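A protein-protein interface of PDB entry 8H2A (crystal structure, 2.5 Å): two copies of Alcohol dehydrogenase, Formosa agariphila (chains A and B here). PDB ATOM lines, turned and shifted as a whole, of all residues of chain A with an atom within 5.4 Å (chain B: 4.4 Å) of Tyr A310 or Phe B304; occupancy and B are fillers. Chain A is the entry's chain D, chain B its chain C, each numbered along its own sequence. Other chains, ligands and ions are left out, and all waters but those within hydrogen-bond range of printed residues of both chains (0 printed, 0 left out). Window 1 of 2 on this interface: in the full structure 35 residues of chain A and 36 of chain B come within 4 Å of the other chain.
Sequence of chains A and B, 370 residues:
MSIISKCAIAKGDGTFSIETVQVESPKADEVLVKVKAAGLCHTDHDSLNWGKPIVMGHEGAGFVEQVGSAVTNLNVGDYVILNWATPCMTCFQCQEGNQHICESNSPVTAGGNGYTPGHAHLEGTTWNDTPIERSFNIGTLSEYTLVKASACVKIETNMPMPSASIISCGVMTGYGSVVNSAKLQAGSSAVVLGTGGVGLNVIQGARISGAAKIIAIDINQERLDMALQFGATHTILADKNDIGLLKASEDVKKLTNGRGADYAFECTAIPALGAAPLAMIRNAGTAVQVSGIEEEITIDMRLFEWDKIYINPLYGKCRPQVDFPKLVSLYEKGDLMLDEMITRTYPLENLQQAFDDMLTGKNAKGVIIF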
ATOM      1  N   GLY A 274       6.069 -21.475 -25.232  1.00  0.00           N
ATOM      2  CA  GLY A 274       4.982 -22.017 -26.036  1.00  0.00           C
ATOM      3  C   GLY A 274       3.983 -20.986 -26.540  1.00  0.00           C
ATOM      4  O   GLY A 274       3.386 -21.175 -27.608  1.00  0.00           O
ATOM      5  N   ALA A 275       3.795 -19.886 -25.801  1.00  0.00           N
ATOM      6  CA  ALA A 275       2.793 -18.879 -26.137  1.00  0.00           C
ATOM      7  C   ALA A 275       3.389 -17.667 -26.830  1.00  0.00           C
ATOM      8  O   ALA A 275       2.677 -16.689 -27.074  1.00  0.00           O
ATOM      9  CB  ALA A 275       2.035 -18.436 -24.881  1.00  0.00           C
ATOM     10  N   PRO A 277       4.584 -16.945 -29.995  1.00  0.00           N
ATOM     11  CA  PRO A 277       4.070 -16.440 -31.281  1.00  0.00           C
ATOM     12  C   PRO A 277       2.887 -15.525 -31.100  1.00  0.00           C
ATOM     13  O   PRO A 277       2.735 -14.565 -31.862  1.00  0.00           O
ATOM     14  CB  PRO A 277       3.677 -17.717 -32.026  1.00  0.00           C
ATOM     15  CG  PRO A 277       4.499 -18.778 -31.403  1.00  0.00           C
ATOM     16  CD  PRO A 277       4.582 -18.421 -29.966  1.00  0.00           C
ATOM     17  N   LEU A 278       2.047 -15.788 -30.087  1.00  0.00           N
ATOM     18  CA  LEU A 278       0.900 -14.916 -29.839  1.00  0.00           C
ATOM     19  C   LEU A 278       1.336 -13.511 -29.445  1.00  0.00           C
ATOM     20  O   LEU A 278       0.653 -12.534 -29.779  1.00  0.00           O
ATOM     21  CB  LEU A 278       0.005 -15.506 -28.761  1.00  0.00           C
ATOM     22  CG  LEU A 278      -0.661 -16.847 -29.078  1.00  0.00           C
ATOM     23  CD1 LEU A 278      -0.884 -17.606 -27.776  1.00  0.00           C
ATOM     24  CD2 LEU A 278      -1.981 -16.701 -29.865  1.00  0.00           C
ATOM     25  N   ALA A 287      -1.048 -17.994 -35.015  1.00  0.00           N
ATOM     26  CA  ALA A 287       0.137 -18.405 -34.271  1.00  0.00           C
ATOM     27  C   ALA A 287       0.302 -19.911 -34.381  1.00  0.00           C
ATOM     28  O   ALA A 287      -0.605 -20.659 -34.018  1.00  0.00           O
ATOM     29  CB  ALA A 287       0.019 -17.994 -32.805  1.00  0.00           C
ATOM     30  N   GLN A 289       2.561 -23.206 -33.414  1.00  0.00           N
ATOM     31  CA  GLN A 289       3.507 -23.756 -32.456  1.00  0.00           C
ATOM     32  C   GLN A 289       3.959 -25.091 -33.029  1.00  0.00           C
ATOM     33  O   GLN A 289       3.239 -26.079 -32.948  1.00  0.00           O
ATOM     34  CB  GLN A 289       2.778 -23.873 -31.130  1.00  0.00           C
ATOM     35  CG  GLN A 289       3.525 -24.038 -29.836  1.00  0.00           C
ATOM     36  CD  GLN A 289       3.741 -25.483 -29.470  1.00  0.00           C
ATOM     37  OE1 GLN A 289       3.700 -26.360 -30.314  1.00  0.00           O
ATOM     38  NE2 GLN A 289       3.829 -25.745 -28.200  1.00  0.00           N
ATOM     39  N   ILE A 299       0.490 -19.552 -19.005  1.00  0.00           N
ATOM     40  CA  ILE A 299       0.281 -18.674 -20.140  1.00  0.00           C
ATOM     41  C   ILE A 299      -0.512 -17.473 -19.658  1.00  0.00           C
ATOM     42  O   ILE A 299      -1.533 -17.628 -18.983  1.00  0.00           O
ATOM     43  CB  ILE A 299      -0.440 -19.390 -21.292  1.00  0.00           C
ATOM     44  CG1 ILE A 299       0.425 -20.557 -21.804  1.00  0.00           C
ATOM     45  CG2 ILE A 299      -0.784 -18.384 -22.398  1.00  0.00           C
ATOM     46  CD1 ILE A 299      -0.022 -21.098 -23.144  1.00  0.00           C
ATOM     47  N   PHE A 304      -3.728 -14.730 -25.793  1.00  0.00           N
ATOM     48  CA  PHE A 304      -4.650 -15.324 -26.754  1.00  0.00           C
ATOM     49  C   PHE A 304      -5.677 -14.326 -27.231  1.00  0.00           C
ATOM     50  O   PHE A 304      -6.270 -14.519 -28.301  1.00  0.00           O
ATOM     51  CB  PHE A 304      -5.378 -16.505 -26.137  1.00  0.00           C
ATOM     52  CG  PHE A 304      -4.585 -17.775 -26.143  1.00  0.00           C
ATOM     53  CD1 PHE A 304      -4.297 -18.423 -27.332  1.00  0.00           C
ATOM     54  CD2 PHE A 304      -4.134 -18.325 -24.957  1.00  0.00           C
ATOM     55  CE1 PHE A 304      -3.593 -19.593 -27.334  1.00  0.00           C
ATOM     56  CE2 PHE A 304      -3.435 -19.492 -24.957  1.00  0.00           C
ATOM     57  CZ  PHE A 304      -3.160 -20.129 -26.152  1.00  0.00           C
ATOM     58  N   LYS A 308      -6.808 -14.503 -32.468  1.00  0.00           N
ATOM     59  CA  LYS A 308      -5.543 -15.118 -32.831  1.00  0.00           C
ATOM     60  C   LYS A 308      -5.749 -16.622 -32.891  1.00  0.00           C
ATOM     61  O   LYS A 308      -6.222 -17.235 -31.929  1.00  0.00           O
ATOM     62  CB  LYS A 308      -4.453 -14.758 -31.826  1.00  0.00           C
ATOM     63  CG  LYS A 308      -4.412 -13.277 -31.478  1.00  0.00           C
ATOM     64  CD  LYS A 308      -3.271 -12.933 -30.525  1.00  0.00           C
ATOM     65  CE  LYS A 308      -2.999 -11.432 -30.514  1.00  0.00           C
ATOM     66  NZ  LYS A 308      -2.228 -10.995 -29.295  1.00  0.00           N
ATOM     67  N   ILE A 309      -5.426 -17.198 -34.036  1.00  0.00           N
ATOM     68  CA  ILE A 309      -5.528 -18.633 -34.259  1.00  0.00           C
ATOM     69  C   ILE A 309      -4.271 -19.264 -33.690  1.00  0.00           C
ATOM     70  O   ILE A 309      -3.159 -18.879 -34.054  1.00  0.00           O
ATOM     71  CB  ILE A 309      -5.683 -18.926 -35.756  1.00  0.00           C
ATOM     72  CG1 ILE A 309      -6.806 -18.041 -36.309  1.00  0.00           C
ATOM     73  CG2 ILE A 309      -5.991 -20.388 -36.003  1.00  0.00           C
ATOM     74  CD1 ILE A 309      -6.937 -18.073 -37.757  1.00  0.00           C
ATOM     75  N   TYR A 310      -4.433 -20.183 -32.757  1.00  0.00           N
ATOM     76  CA  TYR A 310      -3.299 -20.837 -32.126  1.00  0.00           C
ATOM     77  C   TYR A 310      -3.411 -22.320 -32.409  1.00  0.00           C
ATOM     78  O   TYR A 310      -4.426 -22.937 -32.076  1.00  0.00           O
ATOM     79  CB  TYR A 310      -3.262 -20.580 -30.630  1.00  0.00           C
ATOM     80  CG  TYR A 310      -2.011 -21.117 -29.957  1.00  0.00           C
ATOM     81  CD1 TYR A 310      -0.836 -20.356 -29.872  1.00  0.00           C
ATOM     82  CD2 TYR A 310      -2.001 -22.398 -29.410  1.00  0.00           C
ATOM     83  CE1 TYR A 310       0.306 -20.866 -29.230  1.00  0.00           C
ATOM     84  CE2 TYR A 310      -0.875 -22.906 -28.776  1.00  0.00           C
ATOM     85  CZ  TYR A 310       0.272 -22.147 -28.690  1.00  0.00           C
ATOM     86  OH  TYR A 310       1.350 -22.704 -28.056  1.00  0.00           O
ATOM     87  N   ILE A 311      -2.383 -22.884 -33.034  1.00  0.00           N
ATOM     88  CA  ILE A 311      -2.436 -24.253 -33.516  1.00  0.00           C
ATOM     89  C   ILE A 311      -1.050 -24.874 -33.420  1.00  0.00           C
ATOM     90  O   ILE A 311      -0.046 -24.248 -33.779  1.00  0.00           O
ATOM     91  CB  ILE A 311      -3.000 -24.312 -34.950  1.00  0.00           C
ATOM     92  CG1 ILE A 311      -3.043 -25.761 -35.456  1.00  0.00           C
ATOM     93  CG2 ILE A 311      -2.236 -23.396 -35.881  1.00  0.00           C
ATOM     94  CD1 ILE A 311      -4.004 -25.944 -36.664  1.00  0.00           C
ATOM     95  N   ASN A 312      -0.999 -26.101 -32.899  1.00  0.00           N
ATOM     96  CA  ASN A 312       0.228 -26.897 -32.889  1.00  0.00           C
ATOM     97  C   ASN A 312       0.030 -28.113 -33.772  1.00  0.00           C
ATOM     98  O   ASN A 312      -0.618 -29.093 -33.344  1.00  0.00           O
ATOM     99  CB  ASN A 312       0.612 -27.320 -31.465  1.00  0.00           C
ATOM    100  CG  ASN A 312       1.735 -28.383 -31.421  1.00  0.00           C
ATOM    101  OD1 ASN A 312       2.692 -28.357 -32.201  1.00  0.00           O
ATOM    102  ND2 ASN A 312       1.655 -29.252 -30.431  1.00  0.00           N
ATOM    103  N   LEU B 278     -10.095 -27.849 -25.588  1.00  0.00           N
ATOM    104  CA  LEU B 278      -9.158 -28.754 -26.243  1.00  0.00           C
ATOM    105  C   LEU B 278      -9.289 -30.173 -25.716  1.00  0.00           C
ATOM    106  O   LEU B 278      -9.010 -31.128 -26.446  1.00  0.00           O
ATOM    107  CB  LEU B 278      -7.726 -28.257 -26.054  1.00  0.00           C
ATOM    108  CG  LEU B 278      -7.438 -26.810 -26.474  1.00  0.00           C
ATOM    109  CD1 LEU B 278      -6.343 -26.242 -25.603  1.00  0.00           C
ATOM    110  CD2 LEU B 278      -7.045 -26.711 -27.928  1.00  0.00           C
ATOM    111  N   ILE B 299      -1.604 -24.343 -18.192  1.00  0.00           N
ATOM    112  CA  ILE B 299      -2.197 -25.181 -19.226  1.00  0.00           C
ATOM    113  C   ILE B 299      -1.246 -26.336 -19.538  1.00  0.00           C
ATOM    114  O   ILE B 299      -0.050 -26.121 -19.781  1.00  0.00           O
ATOM    115  CB  ILE B 299      -2.491 -24.373 -20.499  1.00  0.00           C
ATOM    116  CG1 ILE B 299      -3.519 -23.265 -20.272  1.00  0.00           C
ATOM    117  CG2 ILE B 299      -3.088 -25.279 -21.525  1.00  0.00           C
ATOM    118  CD1 ILE B 299      -3.437 -22.214 -21.393  1.00  0.00           C
ATOM    119  N   MET B 301       0.048 -28.519 -22.212  1.00  0.00           N
ATOM    120  CA  MET B 301       0.109 -28.365 -23.651  1.00  0.00           C
ATOM    121  C   MET B 301       0.002 -29.690 -24.382  1.00  0.00           C
ATOM    122  O   MET B 301       0.259 -29.725 -25.585  1.00  0.00           O
ATOM    123  CB  MET B 301       1.392 -27.643 -24.046  1.00  0.00           C
ATOM    124  CG  MET B 301       1.740 -26.457 -23.150  1.00  0.00           C
ATOM    125  SD  MET B 301       0.728 -24.991 -23.438  1.00  0.00           S
ATOM    126  CE  MET B 301       0.973 -24.775 -25.196  1.00  0.00           C
ATOM    127  N   ARG B 302      -0.351 -30.788 -23.702  1.00  0.00           N
ATOM    128  CA  ARG B 302      -0.765 -31.985 -24.426  1.00  0.00           C
ATOM    129  C   ARG B 302      -2.194 -31.865 -24.921  1.00  0.00           C
ATOM    130  O   ARG B 302      -2.586 -32.601 -25.835  1.00  0.00           O
ATOM    131  CB  ARG B 302      -0.614 -33.248 -23.570  1.00  0.00           C
ATOM    132  CG  ARG B 302       0.766 -33.397 -23.011  1.00  0.00           C
ATOM    133  CD  ARG B 302       0.842 -34.428 -21.918  1.00  0.00           C
ATOM    134  NE  ARG B 302       1.106 -35.759 -22.459  1.00  0.00           N
ATOM    135  CZ  ARG B 302       0.566 -36.884 -21.993  1.00  0.00           C
ATOM    136  NH1 ARG B 302      -0.269 -36.845 -20.958  1.00  0.00           N
ATOM    137  NH2 ARG B 302       0.883 -38.052 -22.549  1.00  0.00           N
ATOM    138  N   LEU B 303      -2.949 -30.903 -24.399  1.00  0.00           N
ATOM    139  CA  LEU B 303      -4.309 -30.680 -24.879  1.00  0.00           C
ATOM    140  C   LEU B 303      -4.348 -29.969 -26.225  1.00  0.00           C
ATOM    141  O   LEU B 303      -5.247 -30.230 -27.018  1.00  0.00           O
ATOM    142  CB  LEU B 303      -5.102 -29.867 -23.857  1.00  0.00           C
ATOM    143  CG  LEU B 303      -5.109 -30.399 -22.430  1.00  0.00           C
ATOM    144  CD1 LEU B 303      -5.573 -29.301 -21.503  1.00  0.00           C
ATOM    145  CD2 LEU B 303      -5.992 -31.626 -22.325  1.00  0.00           C
ATOM    146  N   PHE B 304      -3.411 -29.048 -26.495  1.00  0.00           N
ATOM    147  CA  PHE B 304      -3.355 -28.370 -27.793  1.00  0.00           C
ATOM    148  C   PHE B 304      -2.991 -29.335 -28.923  1.00  0.00           C
ATOM    149  O   PHE B 304      -3.232 -29.030 -30.102  1.00  0.00           O
ATOM    150  CB  PHE B 304      -2.293 -27.261 -27.786  1.00  0.00           C
ATOM    151  CG  PHE B 304      -2.646 -26.026 -26.986  1.00  0.00           C
ATOM    152  CD1 PHE B 304      -3.272 -24.946 -27.593  1.00  0.00           C
ATOM    153  CD2 PHE B 304      -2.275 -25.918 -25.643  1.00  0.00           C
ATOM    154  CE1 PHE B 304      -3.567 -23.796 -26.861  1.00  0.00           C
ATOM    155  CE2 PHE B 304      -2.560 -24.774 -24.909  1.00  0.00           C
ATOM    156  CZ  PHE B 304      -3.197 -23.711 -25.508  1.00  0.00           C
ATOM    157  N   GLU B 305      -2.408 -30.482 -28.586  1.00  0.00           N
ATOM    158  CA  GLU B 305      -1.583 -31.194 -29.546  1.00  0.00           C
ATOM    159  C   GLU B 305      -2.420 -31.862 -30.617  1.00  0.00           C
ATOM    160  O   GLU B 305      -3.414 -32.538 -30.308  1.00  0.00           O
ATOM    161  CB  GLU B 305      -0.696 -32.216 -28.836  1.00  0.00           C
ATOM    162  CG  GLU B 305       0.640 -31.569 -28.613  1.00  0.00           C
ATOM    163  CD  GLU B 305       1.696 -32.440 -27.994  1.00  0.00           C
ATOM    164  OE1 GLU B 305       1.428 -33.610 -27.671  1.00  0.00           O
ATOM    165  OE2 GLU B 305       2.826 -31.926 -27.850  1.00  0.00           O
ATOM    166  N   TRP B 306      -2.027 -31.589 -31.882  1.00  0.00           N
ATOM    167  CA  TRP B 306      -2.312 -32.439 -33.023  1.00  0.00           C
ATOM    168  C   TRP B 306      -3.454 -31.730 -33.734  1.00  0.00           C
ATOM    169  O   TRP B 306      -4.613 -32.156 -33.686  1.00  0.00           O
ATOM    170  CB  TRP B 306      -2.543 -33.808 -32.406  1.00  0.00           C
ATOM    171  CG  TRP B 306      -1.226 -34.506 -31.909  1.00  0.00           C
ATOM    172  CD1 TRP B 306      -0.967 -35.812 -31.992  1.00  0.00           C
ATOM    173  CD2 TRP B 306       0.120 -33.901 -31.808  1.00  0.00           C
ATOM    174  NE1 TRP B 306       0.295 -36.098 -31.559  1.00  0.00           N
ATOM    175  CE2 TRP B 306       1.011 -34.935 -31.517  1.00  0.00           C
ATOM    176  CE3 TRP B 306       0.621 -32.589 -31.823  1.00  0.00           C
ATOM    177  CZ2 TRP B 306       2.374 -34.709 -31.241  1.00  0.00           C
ATOM    178  CZ3 TRP B 306       1.972 -32.372 -31.551  1.00  0.00           C
ATOM    179  CH2 TRP B 306       2.823 -33.425 -31.255  1.00  0.00           C
ATOM    180  N   LYS B 308      -5.140 -28.980 -33.543  1.00  0.00           N
ATOM    181  CA  LYS B 308      -6.310 -28.379 -32.918  1.00  0.00           C
ATOM    182  C   LYS B 308      -6.301 -26.872 -33.135  1.00  0.00           C
ATOM    183  O   LYS B 308      -5.288 -26.207 -32.917  1.00  0.00           O
ATOM    184  CB  LYS B 308      -6.334 -28.703 -31.424  1.00  0.00           C
ATOM    185  CG  LYS B 308      -6.439 -30.188 -31.120  1.00  0.00           C
ATOM    186  CD  LYS B 308      -7.000 -30.440 -29.732  1.00  0.00           C
ATOM    187  CE  LYS B 308      -6.814 -31.905 -29.347  1.00  0.00           C
ATOM    188  NZ  LYS B 308      -6.995 -32.163 -27.886  1.00  0.00           N
ATOM    189  N   ILE B 309      -7.416 -26.326 -33.595  1.00  0.00           N
ATOM    190  CA  ILE B 309      -7.479 -24.894 -33.846  1.00  0.00           C
ATOM    191  C   ILE B 309      -8.077 -24.205 -32.630  1.00  0.00           C
ATOM    192  O   ILE B 309      -9.268 -24.346 -32.363  1.00  0.00           O
ATOM    193  CB  ILE B 309      -8.282 -24.563 -35.096  1.00  0.00           C
ATOM    194  CG1 ILE B 309      -7.679 -25.264 -36.320  1.00  0.00           C
ATOM    195  CG2 ILE B 309      -8.270 -23.067 -35.257  1.00  0.00           C
ATOM    196  CD1 ILE B 309      -8.677 -25.451 -37.494  1.00  0.00           C
ATOM    197  N   TYR B 310      -7.256 -23.444 -31.917  1.00  0.00           N
ATOM    198  CA  TYR B 310      -7.675 -22.640 -30.783  1.00  0.00           C
ATOM    199  C   TYR B 310      -7.911 -21.189 -31.228  1.00  0.00           C
ATOM    200  O   TYR B 310      -7.264 -20.698 -32.148  1.00  0.00           O
ATOM    201  CB  TYR B 310      -6.603 -22.702 -29.691  1.00  0.00           C
ATOM    202  CG  TYR B 310      -7.041 -22.163 -28.357  1.00  0.00           C
ATOM    203  CD1 TYR B 310      -6.930 -20.812 -28.068  1.00  0.00           C
ATOM    204  CD2 TYR B 310      -7.571 -23.007 -27.384  1.00  0.00           C
ATOM    205  CE1 TYR B 310      -7.330 -20.305 -26.842  1.00  0.00           C
ATOM    206  CE2 TYR B 310      -7.986 -22.518 -26.146  1.00  0.00           C
ATOM    207  CZ  TYR B 310      -7.860 -21.162 -25.881  1.00  0.00           C
ATOM    208  OH  TYR B 310      -8.252 -20.653 -24.664  1.00  0.00           O
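The backbone NH (N) of Trp B306 is in hydrogen-bond range of the backbone carbonyl oxygen (O) of Asn A312 (3.2 Å). N of Tyr B310 sits at hydrogen-bond distance from O of Tyr A310, 2.9 Å away. The backbone carbonyl oxygen (O) of Tyr A310 lies close to the backbone carbonyl oxygen (O) of Lys B308 (3.5 Å).
The backbone carbonyl oxygen (O) of Leu B278 lies within hydrogen-bond range of the side-chain amino group (NZ) of Lys B308 (2.7 Å). The backbone carbonyl oxygen of Leu B303 lies within hydrogen-bond range of the side-chain amino group of Lys B308, 2.7 Å away. The backbone carbonyl oxygen (O) of Gly A274 sits at hydrogen-bond distance from the side-chain hydroxyl (OH) of Tyr A310 (2.6 Å). O of Ala A287 is in hydrogen-bond range of N of Ile A311 (3.0 Å). The backbone NH of Gln A289 lies within hydrogen-bond range of the backbone carbonyl oxygen of Ile A311, at 2.8 Å. The backbone carbonyl oxygen (O) of Gln A289 lies close to the side-chain amide oxygen (OD1) of Asn A312 (2.5 Å).
Among the printed residues, merely in contact across the chains: Asn A312 with Glu B305 (3.1 Å), Tyr A310 with Phe B304 (3.3 Å), Ile A311 with Lys B308 (3.4 Å), Ile A309 with Tyr B310 (3.4 Å), Tyr A310 with Met B301 (3.6 Å), Ile A309 with Ile B309 (3.6 Å), Phe A304 with Tyr B310 (3.6 Å), Lys A308 with Tyr B310 (3.6 Å), Phe A304 with Phe B304 (3.6 Å), Ile A311 with Ile B309 (3.8 Å), Tyr A310 with Ile B309 (3.9 Å), Ile A299 with Met B301 (3.98 Å) and Ile A299 with Ile B299 (3.997 Å).
Gly A274 touches none of the printed residues of chain B. Of the printed residues of chain B, Phe A304 touches Phe B304 and Tyr B310. Of chain B, only Met B301, Phe B304, Lys B308, Ile B309 and Tyr B310 come within 4 Å of Tyr A310. Arg B302 touches none of the printed residues of chain A. Phe B304 touches just these residues of chain A: Phe A304 and Tyr A310. Of the printed residues of chain A, Glu B305 touches Asn A312. The nearest printed residue of chain B that does not touch Tyr A310 is Leu B278 (6.2 Å). The nearest printed residue of chain A that does not touch Ile B309 is Asn A312 (6.5 Å).
Hydrophobic or aromatic side chains of chain A within 4 Å of the printed part of chain B: Ile A299, Phe A304, Ile A309, Tyr A310 and Ile A311. Hydrophobic or aromatic side chains of chain B that line the printed part of chain A: Ile B299, Met B301, Phe B304, Trp B306, Ile B309 and Tyr B310. Among the printed residues, 16 pairs touch across the chains.
Phe A304 touches Tyr B310, and with the chains exchanged Tyr A310 touches Phe B304. Lys A308 touches Tyr B310, and with the chains exchanged Tyr A310 touches Lys B308. Ile A309 touches Tyr B310, and with the chains exchanged Tyr A310 touches Ile B309. Tyr B310 touches its own counterpart, Tyr A310. Of the 16 pairs that touch across the chains among the printed residues, 10 have their exchanged pair printed and touching as well.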
